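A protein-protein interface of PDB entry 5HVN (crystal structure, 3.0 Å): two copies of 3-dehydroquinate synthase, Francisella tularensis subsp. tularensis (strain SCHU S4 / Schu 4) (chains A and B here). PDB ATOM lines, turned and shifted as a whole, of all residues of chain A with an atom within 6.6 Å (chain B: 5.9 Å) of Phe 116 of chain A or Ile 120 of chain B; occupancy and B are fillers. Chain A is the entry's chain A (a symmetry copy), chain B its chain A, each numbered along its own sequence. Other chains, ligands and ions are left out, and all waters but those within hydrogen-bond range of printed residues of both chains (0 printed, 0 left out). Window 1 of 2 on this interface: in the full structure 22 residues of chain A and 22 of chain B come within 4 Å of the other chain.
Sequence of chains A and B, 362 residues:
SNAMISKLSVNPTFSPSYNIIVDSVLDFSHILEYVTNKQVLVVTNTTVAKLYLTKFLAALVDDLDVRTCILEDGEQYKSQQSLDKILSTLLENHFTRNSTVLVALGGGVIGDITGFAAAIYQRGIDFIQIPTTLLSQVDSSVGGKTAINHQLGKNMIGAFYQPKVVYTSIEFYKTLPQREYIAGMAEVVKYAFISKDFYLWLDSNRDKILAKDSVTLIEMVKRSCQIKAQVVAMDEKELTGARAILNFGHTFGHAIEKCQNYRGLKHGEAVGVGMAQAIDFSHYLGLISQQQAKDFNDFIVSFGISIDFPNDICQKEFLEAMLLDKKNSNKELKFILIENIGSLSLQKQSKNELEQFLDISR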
ATOM      1  N   GLN A  80      20.058  -8.173 -17.786  1.00  0.00           N
ATOM      2  CA  GLN A  80      21.020  -8.153 -16.705  1.00  0.00           C
ATOM      3  C   GLN A  80      20.791  -6.866 -15.924  1.00  0.00           C
ATOM      4  O   GLN A  80      20.800  -6.883 -14.694  1.00  0.00           O
ATOM      5  CB  GLN A  80      22.455  -8.213 -17.223  1.00  0.00           C
ATOM      6  CG  GLN A  80      23.500  -8.190 -16.119  1.00  0.00           C
ATOM      7  CD  GLN A  80      23.427  -9.415 -15.226  1.00  0.00           C
ATOM      8  OE1 GLN A  80      23.388 -10.547 -15.715  1.00  0.00           O
ATOM      9  NE2 GLN A  80      23.437  -9.197 -13.912  1.00  0.00           N
ATOM     10  N   LEU A  83      18.107  -7.437 -13.557  1.00  0.00           N
ATOM     11  CA  LEU A  83      18.566  -8.409 -12.585  1.00  0.00           C
ATOM     12  C   LEU A  83      19.379  -7.698 -11.497  1.00  0.00           C
ATOM     13  O   LEU A  83      19.214  -7.996 -10.319  1.00  0.00           O
ATOM     14  CB  LEU A  83      19.383  -9.494 -13.268  1.00  0.00           C
ATOM     15  CG  LEU A  83      19.976 -10.579 -12.372  1.00  0.00           C
ATOM     16  CD1 LEU A  83      18.880 -11.319 -11.613  1.00  0.00           C
ATOM     17  CD2 LEU A  83      20.843 -11.532 -13.198  1.00  0.00           C
ATOM     18  N   LEU A 102      11.625 -14.311  -2.593  1.00  0.00           N
ATOM     19  CA  LEU A 102      11.316 -13.456  -3.705  1.00  0.00           C
ATOM     20  C   LEU A 102       9.922 -13.881  -4.153  1.00  0.00           C
ATOM     21  O   LEU A 102       9.619 -15.086  -4.243  1.00  0.00           O
ATOM     22  CB  LEU A 102      12.305 -13.614  -4.850  1.00  0.00           C
ATOM     23  CG  LEU A 102      13.682 -13.021  -4.681  1.00  0.00           C
ATOM     24  CD1 LEU A 102      14.468 -13.196  -5.960  1.00  0.00           C
ATOM     25  CD2 LEU A 102      13.530 -11.545  -4.416  1.00  0.00           C
ATOM     26  N   GLY A 111       8.247 -13.656 -13.968  1.00  0.00           N
ATOM     27  CA  GLY A 111       8.506 -15.007 -13.461  1.00  0.00           C
ATOM     28  C   GLY A 111       9.915 -15.528 -13.762  1.00  0.00           C
ATOM     29  O   GLY A 111      10.541 -16.150 -12.915  1.00  0.00           O
ATOM     30  N   ASP A 112      10.425 -15.255 -14.958  1.00  0.00           N
ATOM     31  CA  ASP A 112      11.746 -15.725 -15.345  1.00  0.00           C
ATOM     32  C   ASP A 112      12.853 -15.060 -14.614  1.00  0.00           C
ATOM     33  O   ASP A 112      13.744 -15.748 -14.086  1.00  0.00           O
ATOM     34  CB  ASP A 112      12.003 -15.578 -16.853  1.00  0.00           C
ATOM     35  CG  ASP A 112      11.419 -16.717 -17.672  1.00  0.00           C
ATOM     36  OD1 ASP A 112      10.308 -17.205 -17.353  1.00  0.00           O
ATOM     37  OD2 ASP A 112      12.078 -17.117 -18.656  1.00  0.00           O
ATOM     38  N   ILE A 113      12.814 -13.724 -14.598  1.00  0.00           N
ATOM     39  CA  ILE A 113      13.877 -12.933 -13.962  1.00  0.00           C
ATOM     40  C   ILE A 113      13.894 -13.112 -12.434  1.00  0.00           C
ATOM     41  O   ILE A 113      14.969 -13.303 -11.852  1.00  0.00           O
ATOM     42  CB  ILE A 113      13.862 -11.461 -14.422  1.00  0.00           C
ATOM     43  CG1 ILE A 113      15.155 -10.763 -14.051  1.00  0.00           C
ATOM     44  CG2 ILE A 113      12.653 -10.726 -13.892  1.00  0.00           C
ATOM     45  CD1 ILE A 113      15.296  -9.395 -14.686  1.00  0.00           C
ATOM     46  N   THR A 114      12.714 -13.107 -11.813  1.00  0.00           N
ATOM     47  CA  THR A 114      12.598 -13.281 -10.389  1.00  0.00           C
ATOM     48  C   THR A 114      13.092 -14.663 -10.021  1.00  0.00           C
ATOM     49  O   THR A 114      13.845 -14.814  -9.055  1.00  0.00           O
ATOM     50  CB  THR A 114      11.164 -13.043  -9.914  1.00  0.00           C
ATOM     51  OG1 THR A 114      10.797 -11.697 -10.234  1.00  0.00           O
ATOM     52  CG2 THR A 114      11.031 -13.232  -8.406  1.00  0.00           C
ATOM     53  N   GLY A 115      12.695 -15.672 -10.787  1.00  0.00           N
ATOM     54  CA  GLY A 115      13.145 -17.046 -10.523  1.00  0.00           C
ATOM     55  C   GLY A 115      14.665 -17.156 -10.633  1.00  0.00           C
ATOM     56  O   GLY A 115      15.322 -17.792  -9.794  1.00  0.00           O
ATOM     57  N   PHE A 116      15.229 -16.512 -11.658  1.00  0.00           N
ATOM     58  CA  PHE A 116      16.661 -16.548 -11.858  1.00  0.00           C
ATOM     59  C   PHE A 116      17.375 -15.865 -10.704  1.00  0.00           C
ATOM     60  O   PHE A 116      18.355 -16.415 -10.181  1.00  0.00           O
ATOM     61  CB  PHE A 116      17.065 -15.986 -13.219  1.00  0.00           C
ATOM     62  CG  PHE A 116      18.547 -16.042 -13.480  1.00  0.00           C
ATOM     63  CD1 PHE A 116      19.234 -17.270 -13.456  1.00  0.00           C
ATOM     64  CD2 PHE A 116      19.259 -14.879 -13.812  1.00  0.00           C
ATOM     65  CE1 PHE A 116      20.619 -17.329 -13.705  1.00  0.00           C
ATOM     66  CE2 PHE A 116      20.631 -14.934 -14.073  1.00  0.00           C
ATOM     67  CZ  PHE A 116      21.311 -16.166 -14.021  1.00  0.00           C
ATOM     68  N   ALA A 117      16.876 -14.689 -10.299  1.00  0.00           N
ATOM     69  CA  ALA A 117      17.448 -13.943  -9.160  1.00  0.00           C
ATOM     70  C   ALA A 117      17.451 -14.838  -7.920  1.00  0.00           C
ATOM     71  O   ALA A 117      18.494 -15.009  -7.284  1.00  0.00           O
ATOM     72  CB  ALA A 117      16.686 -12.658  -8.899  1.00  0.00           C
ATOM     73  N   ALA A 118      16.298 -15.441  -7.619  1.00  0.00           N
ATOM     74  CA  ALA A 118      16.149 -16.350  -6.489  1.00  0.00           C
ATOM     75  C   ALA A 118      17.104 -17.548  -6.583  1.00  0.00           C
ATOM     76  O   ALA A 118      17.542 -18.095  -5.566  1.00  0.00           O
ATOM     77  CB  ALA A 118      14.723 -16.841  -6.405  1.00  0.00           C
ATOM     78  N   ALA A 119      17.429 -17.957  -7.801  1.00  0.00           N
ATOM     79  CA  ALA A 119      18.308 -19.096  -7.982  1.00  0.00           C
ATOM     80  C   ALA A 119      19.787 -18.791  -7.696  1.00  0.00           C
ATOM     81  O   ALA A 119      20.553 -19.691  -7.341  1.00  0.00           O
ATOM     82  CB  ALA A 119      18.147 -19.647  -9.391  1.00  0.00           C
ATOM     83  N   ILE A 120      20.175 -17.526  -7.834  1.00  0.00           N
ATOM     84  CA  ILE A 120      21.578 -17.146  -7.697  1.00  0.00           C
ATOM     85  C   ILE A 120      21.936 -16.364  -6.456  1.00  0.00           C
ATOM     86  O   ILE A 120      23.091 -16.430  -5.981  1.00  0.00           O
ATOM     87  CB  ILE A 120      22.107 -16.450  -8.979  1.00  0.00           C
ATOM     88  CG1 ILE A 120      21.348 -15.150  -9.268  1.00  0.00           C
ATOM     89  CG2 ILE A 120      22.025 -17.419 -10.162  1.00  0.00           C
ATOM     90  CD1 ILE A 120      21.934 -14.321 -10.391  1.00  0.00           C
ATOM     91  N   TYR A 121      20.955 -15.629  -5.927  1.00  0.00           N
ATOM     92  CA  TYR A 121      21.150 -14.844  -4.709  1.00  0.00           C
ATOM     93  C   TYR A 121      21.566 -15.774  -3.575  1.00  0.00           C
ATOM     94  O   TYR A 121      20.778 -16.595  -3.106  1.00  0.00           O
ATOM     95  CB  TYR A 121      19.904 -14.061  -4.323  1.00  0.00           C
ATOM     96  CG  TYR A 121      20.222 -13.105  -3.218  1.00  0.00           C
ATOM     97  CD1 TYR A 121      21.015 -11.989  -3.472  1.00  0.00           C
ATOM     98  CD2 TYR A 121      19.764 -13.308  -1.915  1.00  0.00           C
ATOM     99  CE1 TYR A 121      21.346 -11.100  -2.473  1.00  0.00           C
ATOM    100  CE2 TYR A 121      20.086 -12.409  -0.911  1.00  0.00           C
ATOM    101  CZ  TYR A 121      20.883 -11.313  -1.212  1.00  0.00           C
ATOM    102  OH  TYR A 121      21.222 -10.398  -0.283  1.00  0.00           O
ATOM    103  N   PHE A 127      11.572 -18.957  -3.525  1.00  0.00           N
ATOM    104  CA  PHE A 127      10.941 -18.320  -4.665  1.00  0.00           C
ATOM    105  C   PHE A 127       9.446 -18.644  -4.694  1.00  0.00           C
ATOM    106  O   PHE A 127       9.056 -19.796  -4.541  1.00  0.00           O
ATOM    107  CB  PHE A 127      11.681 -18.832  -5.887  1.00  0.00           C
ATOM    108  CG  PHE A 127      11.045 -18.510  -7.196  1.00  0.00           C
ATOM    109  CD1 PHE A 127      10.740 -17.196  -7.549  1.00  0.00           C
ATOM    110  CD2 PHE A 127      10.869 -19.523  -8.135  1.00  0.00           C
ATOM    111  CE1 PHE A 127      10.177 -16.916  -8.785  1.00  0.00           C
ATOM    112  CE2 PHE A 127      10.329 -19.252  -9.376  1.00  0.00           C
ATOM    113  CZ  PHE A 127       9.979 -17.947  -9.705  1.00  0.00           C
ATOM    114  N   THR A 146      14.119 -20.821 -15.501  1.00  0.00           N
ATOM    115  CA  THR A 146      14.225 -19.407 -15.177  1.00  0.00           C
ATOM    116  C   THR A 146      15.320 -18.938 -16.120  1.00  0.00           C
ATOM    117  O   THR A 146      16.215 -19.740 -16.471  1.00  0.00           O
ATOM    118  CB  THR A 146      14.641 -19.143 -13.710  1.00  0.00           C
ATOM    119  OG1 THR A 146      16.052 -19.373 -13.533  1.00  0.00           O
ATOM    120  CG2 THR A 146      13.836 -19.994 -12.751  1.00  0.00           C
ATOM    121  N   ALA A 147      15.266 -17.668 -16.534  1.00  0.00           N
ATOM    122  CA  ALA A 147      16.276 -17.118 -17.443  1.00  0.00           C
ATOM    123  C   ALA A 147      16.178 -15.619 -17.606  1.00  0.00           C
ATOM    124  O   ALA A 147      15.228 -14.996 -17.142  1.00  0.00           O
ATOM    125  CB  ALA A 147      16.150 -17.771 -18.809  1.00  0.00           C
ATOM    126  N   ILE A 148      17.198 -15.046 -18.238  1.00  0.00           N
ATOM    127  CA  ILE A 148      17.232 -13.624 -18.591  1.00  0.00           C
ATOM    128  C   ILE A 148      17.796 -13.521 -20.001  1.00  0.00           C
ATOM    129  O   ILE A 148      18.451 -14.449 -20.487  1.00  0.00           O
ATOM    130  CB  ILE A 148      18.068 -12.728 -17.647  1.00  0.00           C
ATOM    131  CG1 ILE A 148      19.529 -13.147 -17.630  1.00  0.00           C
ATOM    132  CG2 ILE A 148      17.485 -12.718 -16.245  1.00  0.00           C
ATOM    133  CD1 ILE A 148      20.436 -12.050 -17.126  1.00  0.00           C
ATOM    134  N   MET A 156      19.294 -17.109 -22.769  1.00  0.00           N
ATOM    135  CA  MET A 156      20.587 -17.789 -22.885  1.00  0.00           C
ATOM    136  C   MET A 156      21.317 -17.980 -21.566  1.00  0.00           C
ATOM    137  O   MET A 156      22.274 -18.745 -21.472  1.00  0.00           O
ATOM    138  CB  MET A 156      21.485 -16.978 -23.824  1.00  0.00           C
ATOM    139  CG  MET A 156      21.111 -17.035 -25.305  1.00  0.00           C
ATOM    140  SD  MET A 156      21.327 -18.698 -25.960  1.00  0.00           S
ATOM    141  CE  MET A 156      21.293 -18.343 -27.726  1.00  0.00           C
ATOM    142  N   ILE A 157      20.866 -17.250 -20.559  1.00  0.00           N
ATOM    143  CA  ILE A 157      21.429 -17.269 -19.238  1.00  0.00           C
ATOM    144  C   ILE A 157      20.262 -17.586 -18.325  1.00  0.00           C
ATOM    145  O   ILE A 157      19.218 -16.933 -18.397  1.00  0.00           O
ATOM    146  CB  ILE A 157      21.961 -15.874 -18.906  1.00  0.00           C
ATOM    147  CG1 ILE A 157      23.064 -15.487 -19.881  1.00  0.00           C
ATOM    148  CG2 ILE A 157      22.461 -15.810 -17.473  1.00  0.00           C
ATOM    149  CD1 ILE A 157      23.422 -14.016 -19.806  1.00  0.00           C
ATOM    150  N   GLY A 158      20.425 -18.585 -17.465  1.00  0.00           N
ATOM    151  CA  GLY A 158      19.352 -18.963 -16.560  1.00  0.00           C
ATOM    152  C   GLY A 158      19.699 -20.112 -15.639  1.00  0.00           C
ATOM    153  O   GLY A 158      20.858 -20.498 -15.525  1.00  0.00           O
ATOM    154  N   ALA A 159      18.684 -20.649 -14.967  1.00  0.00           N
ATOM    155  CA  ALA A 159      18.878 -21.756 -14.053  1.00  0.00           C
ATOM    156  C   ALA A 159      17.602 -22.558 -13.904  1.00  0.00           C
ATOM    157  O   ALA A 159      16.512 -22.057 -14.214  1.00  0.00           O
ATOM    158  CB  ALA A 159      19.300 -21.224 -12.693  1.00  0.00           C
ATOM    159  N   TYR A 161      15.148 -23.765 -11.379  1.00  0.00           N
ATOM    160  CA  TYR A 161      14.825 -23.450  -9.990  1.00  0.00           C
ATOM    161  C   TYR A 161      13.326 -23.585  -9.738  1.00  0.00           C
ATOM    162  O   TYR A 161      12.512 -22.909 -10.362  1.00  0.00           O
ATOM    163  CB  TYR A 161      15.326 -22.048  -9.658  1.00  0.00           C
ATOM    164  CG  TYR A 161      15.610 -21.853  -8.197  1.00  0.00           C
ATOM    165  CD1 TYR A 161      16.742 -22.459  -7.609  1.00  0.00           C
ATOM    166  CD2 TYR A 161      14.790 -21.039  -7.398  1.00  0.00           C
ATOM    167  CE1 TYR A 161      17.025 -22.293  -6.268  1.00  0.00           C
ATOM    168  CE2 TYR A 161      15.075 -20.854  -6.049  1.00  0.00           C
ATOM    169  CZ  TYR A 161      16.190 -21.490  -5.484  1.00  0.00           C
ATOM    170  OH  TYR A 161      16.491 -21.325  -4.145  1.00  0.00           O
ATOM    171  N   LEU B  83      32.120 -11.485 -15.796  1.00  0.00           N
ATOM    172  CA  LEU B  83      31.179 -12.532 -16.139  1.00  0.00           C
ATOM    173  C   LEU B  83      30.600 -12.262 -17.533  1.00  0.00           C
ATOM    174  O   LEU B  83      30.474 -13.185 -18.331  1.00  0.00           O
ATOM    175  CB  LEU B  83      30.082 -12.620 -15.091  1.00  0.00           C
ATOM    176  CG  LEU B  83      28.982 -13.653 -15.327  1.00  0.00           C
ATOM    177  CD1 LEU B  83      29.565 -15.059 -15.416  1.00  0.00           C
ATOM    178  CD2 LEU B  83      27.913 -13.546 -14.237  1.00  0.00           C
ATOM    179  N   LEU B  87      30.496 -14.528 -20.942  1.00  0.00           N
ATOM    180  CA  LEU B  87      29.232 -14.777 -21.602  1.00  0.00           C
ATOM    181  C   LEU B  87      29.183 -14.264 -23.059  1.00  0.00           C
ATOM    182  O   LEU B  87      28.587 -14.918 -23.922  1.00  0.00           O
ATOM    183  CB  LEU B  87      28.075 -14.240 -20.766  1.00  0.00           C
ATOM    184  CG  LEU B  87      27.855 -14.936 -19.436  1.00  0.00           C
ATOM    185  CD1 LEU B  87      26.772 -14.194 -18.689  1.00  0.00           C
ATOM    186  CD2 LEU B  87      27.502 -16.409 -19.603  1.00  0.00           C
ATOM    187  N   GLY B 115      33.229 -21.257 -12.954  1.00  0.00           N
ATOM    188  CA  GLY B 115      32.219 -22.220 -12.490  1.00  0.00           C
ATOM    189  C   GLY B 115      30.818 -21.611 -12.536  1.00  0.00           C
ATOM    190  O   GLY B 115      29.854 -22.258 -12.975  1.00  0.00           O
ATOM    191  N   PHE B 116      30.708 -20.352 -12.104  1.00  0.00           N
ATOM    192  CA  PHE B 116      29.431 -19.677 -12.103  1.00  0.00           C
ATOM    193  C   PHE B 116      28.921 -19.504 -13.523  1.00  0.00           C
ATOM    194  O   PHE B 116      27.743 -19.784 -13.787  1.00  0.00           O
ATOM    195  CB  PHE B 116      29.475 -18.364 -11.326  1.00  0.00           C
ATOM    196  CG  PHE B 116      28.150 -17.649 -11.271  1.00  0.00           C
ATOM    197  CD1 PHE B 116      27.019 -18.278 -10.716  1.00  0.00           C
ATOM    198  CD2 PHE B 116      28.033 -16.323 -11.714  1.00  0.00           C
ATOM    199  CE1 PHE B 116      25.779 -17.613 -10.656  1.00  0.00           C
ATOM    200  CE2 PHE B 116      26.808 -15.654 -11.644  1.00  0.00           C
ATOM    201  CZ  PHE B 116      25.678 -16.303 -11.111  1.00  0.00           C
ATOM    202  N   ALA B 117      29.804 -19.068 -14.430  1.00  0.00           N
ATOM    203  CA  ALA B 117      29.451 -18.900 -15.855  1.00  0.00           C
ATOM    204  C   ALA B 117      28.917 -20.224 -16.404  1.00  0.00           C
ATOM    205  O   ALA B 117      27.824 -20.260 -16.974  1.00  0.00           O
ATOM    206  CB  ALA B 117      30.637 -18.414 -16.668  1.00  0.00           C
ATOM    207  N   ALA B 118      29.668 -21.305 -16.180  1.00  0.00           N
ATOM    208  CA  ALA B 118      29.280 -22.643 -16.609  1.00  0.00           C
ATOM    209  C   ALA B 118      27.935 -23.075 -16.007  1.00  0.00           C
ATOM    210  O   ALA B 118      27.182 -23.843 -16.614  1.00  0.00           O
ATOM    211  CB  ALA B 118      30.351 -23.640 -16.230  1.00  0.00           C
ATOM    212  N   ALA B 119      27.631 -22.582 -14.815  1.00  0.00           N
ATOM    213  CA  ALA B 119      26.390 -22.955 -14.163  1.00  0.00           C
ATOM    214  C   ALA B 119      25.147 -22.273 -14.757  1.00  0.00           C
ATOM    215  O   ALA B 119      24.038 -22.807 -14.666  1.00  0.00           O
ATOM    216  CB  ALA B 119      26.488 -22.664 -12.674  1.00  0.00           C
ATOM    217  N   ILE B 120      25.339 -21.110 -15.376  1.00  0.00           N
ATOM    218  CA  ILE B 120      24.215 -20.325 -15.875  1.00  0.00           C
ATOM    219  C   ILE B 120      24.057 -20.274 -17.376  1.00  0.00           C
ATOM    220  O   ILE B 120      22.927 -20.100 -17.884  1.00  0.00           O
ATOM    221  CB  ILE B 120      24.193 -18.904 -15.254  1.00  0.00           C
ATOM    222  CG1 ILE B 120      25.452 -18.109 -15.617  1.00  0.00           C
ATOM    223  CG2 ILE B 120      24.018 -19.008 -13.735  1.00  0.00           C
ATOM    224  CD1 ILE B 120      25.412 -16.652 -15.206  1.00  0.00           C
ATOM    225  N   TYR B 121      25.176 -20.427 -18.086  1.00  0.00           N
ATOM    226  CA  TYR B 121      25.168 -20.429 -19.549  1.00  0.00           C
ATOM    227  C   TYR B 121      24.263 -21.551 -20.043  1.00  0.00           C
ATOM    228  O   TYR B 121      24.570 -22.731 -19.887  1.00  0.00           O
ATOM    229  CB  TYR B 121      26.566 -20.580 -20.131  1.00  0.00           C
ATOM    230  CG  TYR B 121      26.532 -20.345 -21.608  1.00  0.00           C
ATOM    231  CD1 TYR B 121      26.312 -19.061 -22.101  1.00  0.00           C
ATOM    232  CD2 TYR B 121      26.693 -21.387 -22.522  1.00  0.00           C
ATOM    233  CE1 TYR B 121      26.254 -18.813 -23.455  1.00  0.00           C
ATOM    234  CE2 TYR B 121      26.645 -21.137 -23.885  1.00  0.00           C
ATOM    235  CZ  TYR B 121      26.421 -19.841 -24.329  1.00  0.00           C
ATOM    236  OH  TYR B 121      26.374 -19.532 -25.639  1.00  0.00           O
ATOM    237  N   GLN B 122      23.128 -21.153 -20.608  1.00  0.00           N
ATOM    238  CA  GLN B 122      22.096 -22.074 -21.101  1.00  0.00           C
ATOM    239  C   GLN B 122      21.719 -23.094 -20.019  1.00  0.00           C
ATOM    240  O   GLN B 122      21.577 -24.314 -20.281  1.00  0.00           O
ATOM    241  CB  GLN B 122      22.499 -22.700 -22.428  1.00  0.00           C
ATOM    242  CG  GLN B 122      22.824 -21.613 -23.417  1.00  0.00           C
ATOM    243  CD  GLN B 122      22.803 -22.080 -24.840  1.00  0.00           C
ATOM    244  OE1 GLN B 122      21.880 -22.768 -25.261  1.00  0.00           O
ATOM    245  NE2 GLN B 122      23.798 -21.667 -25.610  1.00  0.00           N
ATOM    246  N   ARG B 123      21.577 -22.545 -18.803  1.00  0.00           N
ATOM    247  CA  ARG B 123      21.240 -23.265 -17.583  1.00  0.00           C
ATOM    248  C   ARG B 123      22.186 -24.427 -17.285  1.00  0.00           C
ATOM    249  O   ARG B 123      21.743 -25.471 -16.815  1.00  0.00           O
ATOM    250  CB  ARG B 123      19.793 -23.752 -17.607  1.00  0.00           C
ATOM    251  CG  ARG B 123      18.801 -22.652 -17.895  1.00  0.00           C
ATOM    252  CD  ARG B 123      17.368 -23.149 -17.812  1.00  0.00           C
ATOM    253  NE  ARG B 123      16.445 -22.096 -18.220  1.00  0.00           N
ATOM    254  CZ  ARG B 123      16.031 -21.917 -19.470  1.00  0.00           C
ATOM    255  NH1 ARG B 123      16.451 -22.731 -20.417  1.00  0.00           N
ATOM    256  NH2 ARG B 123      15.194 -20.931 -19.767  1.00  0.00           N
ATOM    257  N   GLY B 124      23.477 -24.263 -17.580  1.00  0.00           N
ATOM    258  CA  GLY B 124      24.471 -25.323 -17.295  1.00  0.00           C
ATOM    259  C   GLY B 124      25.176 -26.047 -18.438  1.00  0.00           C
ATOM    260  O   GLY B 124      24.546 -26.715 -19.254  1.00  0.00           O
ATOM    261  N   ILE B 125      26.496 -25.912 -18.483  1.00  0.00           N
ATOM    262  CA  ILE B 125      27.335 -26.564 -19.483  1.00  0.00           C
ATOM    263  C   ILE B 125      28.536 -27.167 -18.755  1.00  0.00           C
ATOM    264  O   ILE B 125      28.830 -26.754 -17.631  1.00  0.00           O
ATOM    265  CB  ILE B 125      27.840 -25.587 -20.567  1.00  0.00           C
ATOM    266  CG1 ILE B 125      28.503 -24.376 -19.914  1.00  0.00           C
ATOM    267  CG2 ILE B 125      26.706 -25.168 -21.498  1.00  0.00           C
ATOM    268  CD1 ILE B 125      29.357 -23.565 -20.857  1.00  0.00           C
ATOM    269  N   ALA B 159      26.310 -20.165  -7.563  1.00  0.00           N
ATOM    270  CA  ALA B 159      25.558 -21.390  -7.751  1.00  0.00           C
ATOM    271  C   ALA B 159      26.357 -22.586  -7.278  1.00  0.00           C
ATOM    272  O   ALA B 159      27.587 -22.503  -7.149  1.00  0.00           O
ATOM    273  CB  ALA B 159      25.223 -21.559  -9.223  1.00  0.00           C
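The side-chain hydroxyl of Tyr 121 of chain B is in hydrogen-bond range of the side-chain amide nitrogen of Gln 122 of chain B (3.3 Å). The backbone carbonyl oxygen of Asp 112 of chain A sits at hydrogen-bond distance from the backbone NH of Ala 147 of chain A (3.5 Å). OG1 of Thr 146 of chain A sits at hydrogen-bond distance from O of Ala 159 of chain A. The backbone NH (N) of Ile 148 of chain A sits at hydrogen-bond distance from the backbone carbonyl oxygen (O) of Ile 157 of chain A (2.8 Å).
Among the printed residues, merely in contact across the chains: Ala 147 of chain A with Arg 123 of chain B (3.4 Å), Gly 158 of chain A with Arg 123 of chain B (3.5 Å), Ile 157 of chain A with Ile 120 of chain B (3.5 Å), Ile 157 of chain A with Leu 87 of chain B (3.5 Å), Ala 159 of chain A with Arg 123 of chain B (3.5 Å), Met 156 of chain A with Tyr 121 of chain B (3.7 Å), Phe 116 of chain A with Ile 120 of chain B (3.8 Å), Ile 120 of chain A with Phe 116 of chain B (3.8 Å) and Met 156 of chain A with Ile 120 of chain B (3.9 Å).
The backbone carbonyl oxygen (O) of Ile 120 of chain B is in hydrogen-bond range of the backbone NH (N) of Gly 158 of chain A (3.0 Å). The backbone NH of Gln 122 of chain B is in hydrogen-bond range of the backbone carbonyl oxygen of Met 156 of chain A. The backbone carbonyl oxygen of Thr 146 of chain A sits at hydrogen-bond distance from the guanidinium group of Arg 123 of chain B.
Phe 116 of chain A touches just one residue of chain B: Ile 120. Of the printed residues of chain B, Met 156 of chain A touches Ile 120 (3.9 Å), Tyr 121 (3.7 Å) and Gln 122 (2.7 Å). Of the printed residues of chain B, Gly 158 of chain A touches Ile 120 and Arg 123. Printed residues of chain B within 4 Å of Ala 159 of chain A: Arg 123 (3.5 Å). Of chain A, only Phe 116, Met 156, Ile 157 and Gly 158 come within 4 Å of Ile 120 of chain B. The nearest residue of chain A that does not touch Ile 120 of chain B is Ile 120 of chain A (4.4 Å). The nearest printed residue of chain A that does not touch Gln 122 of chain B is Ile 157 of chain A (4.5 Å).
Of the 14 printed residues of chain B, 6 touch a printed residue of chain A. Hydrophobic or aromatic side chains of chain B within 4 Å of the printed part of chain A: Leu 87, Phe 116 and Ile 120. Along chain B the printed residues that touch a printed residue of chain A span positions 87 to 123. Of the 23 printed residues of chain A, 8 touch a printed residue of chain B. Hydrophobic or aromatic side chains of chain A that line the printed part of chain B: Phe 116, Ile 120, Ala 147, Met 156 and Ile 157.
Phe 116 of chain A touches Ile 120 of chain B, and with the chains exchanged Ile 120 of chain A touches Phe 116 of chain B. Positions printed for both chains: 83, 115, 116, 117, 118, 119, 120, 121 and 159. Of the 12 pairs that touch across the chains among the printed residues, 2 have their exchanged pair printed and touching as well.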
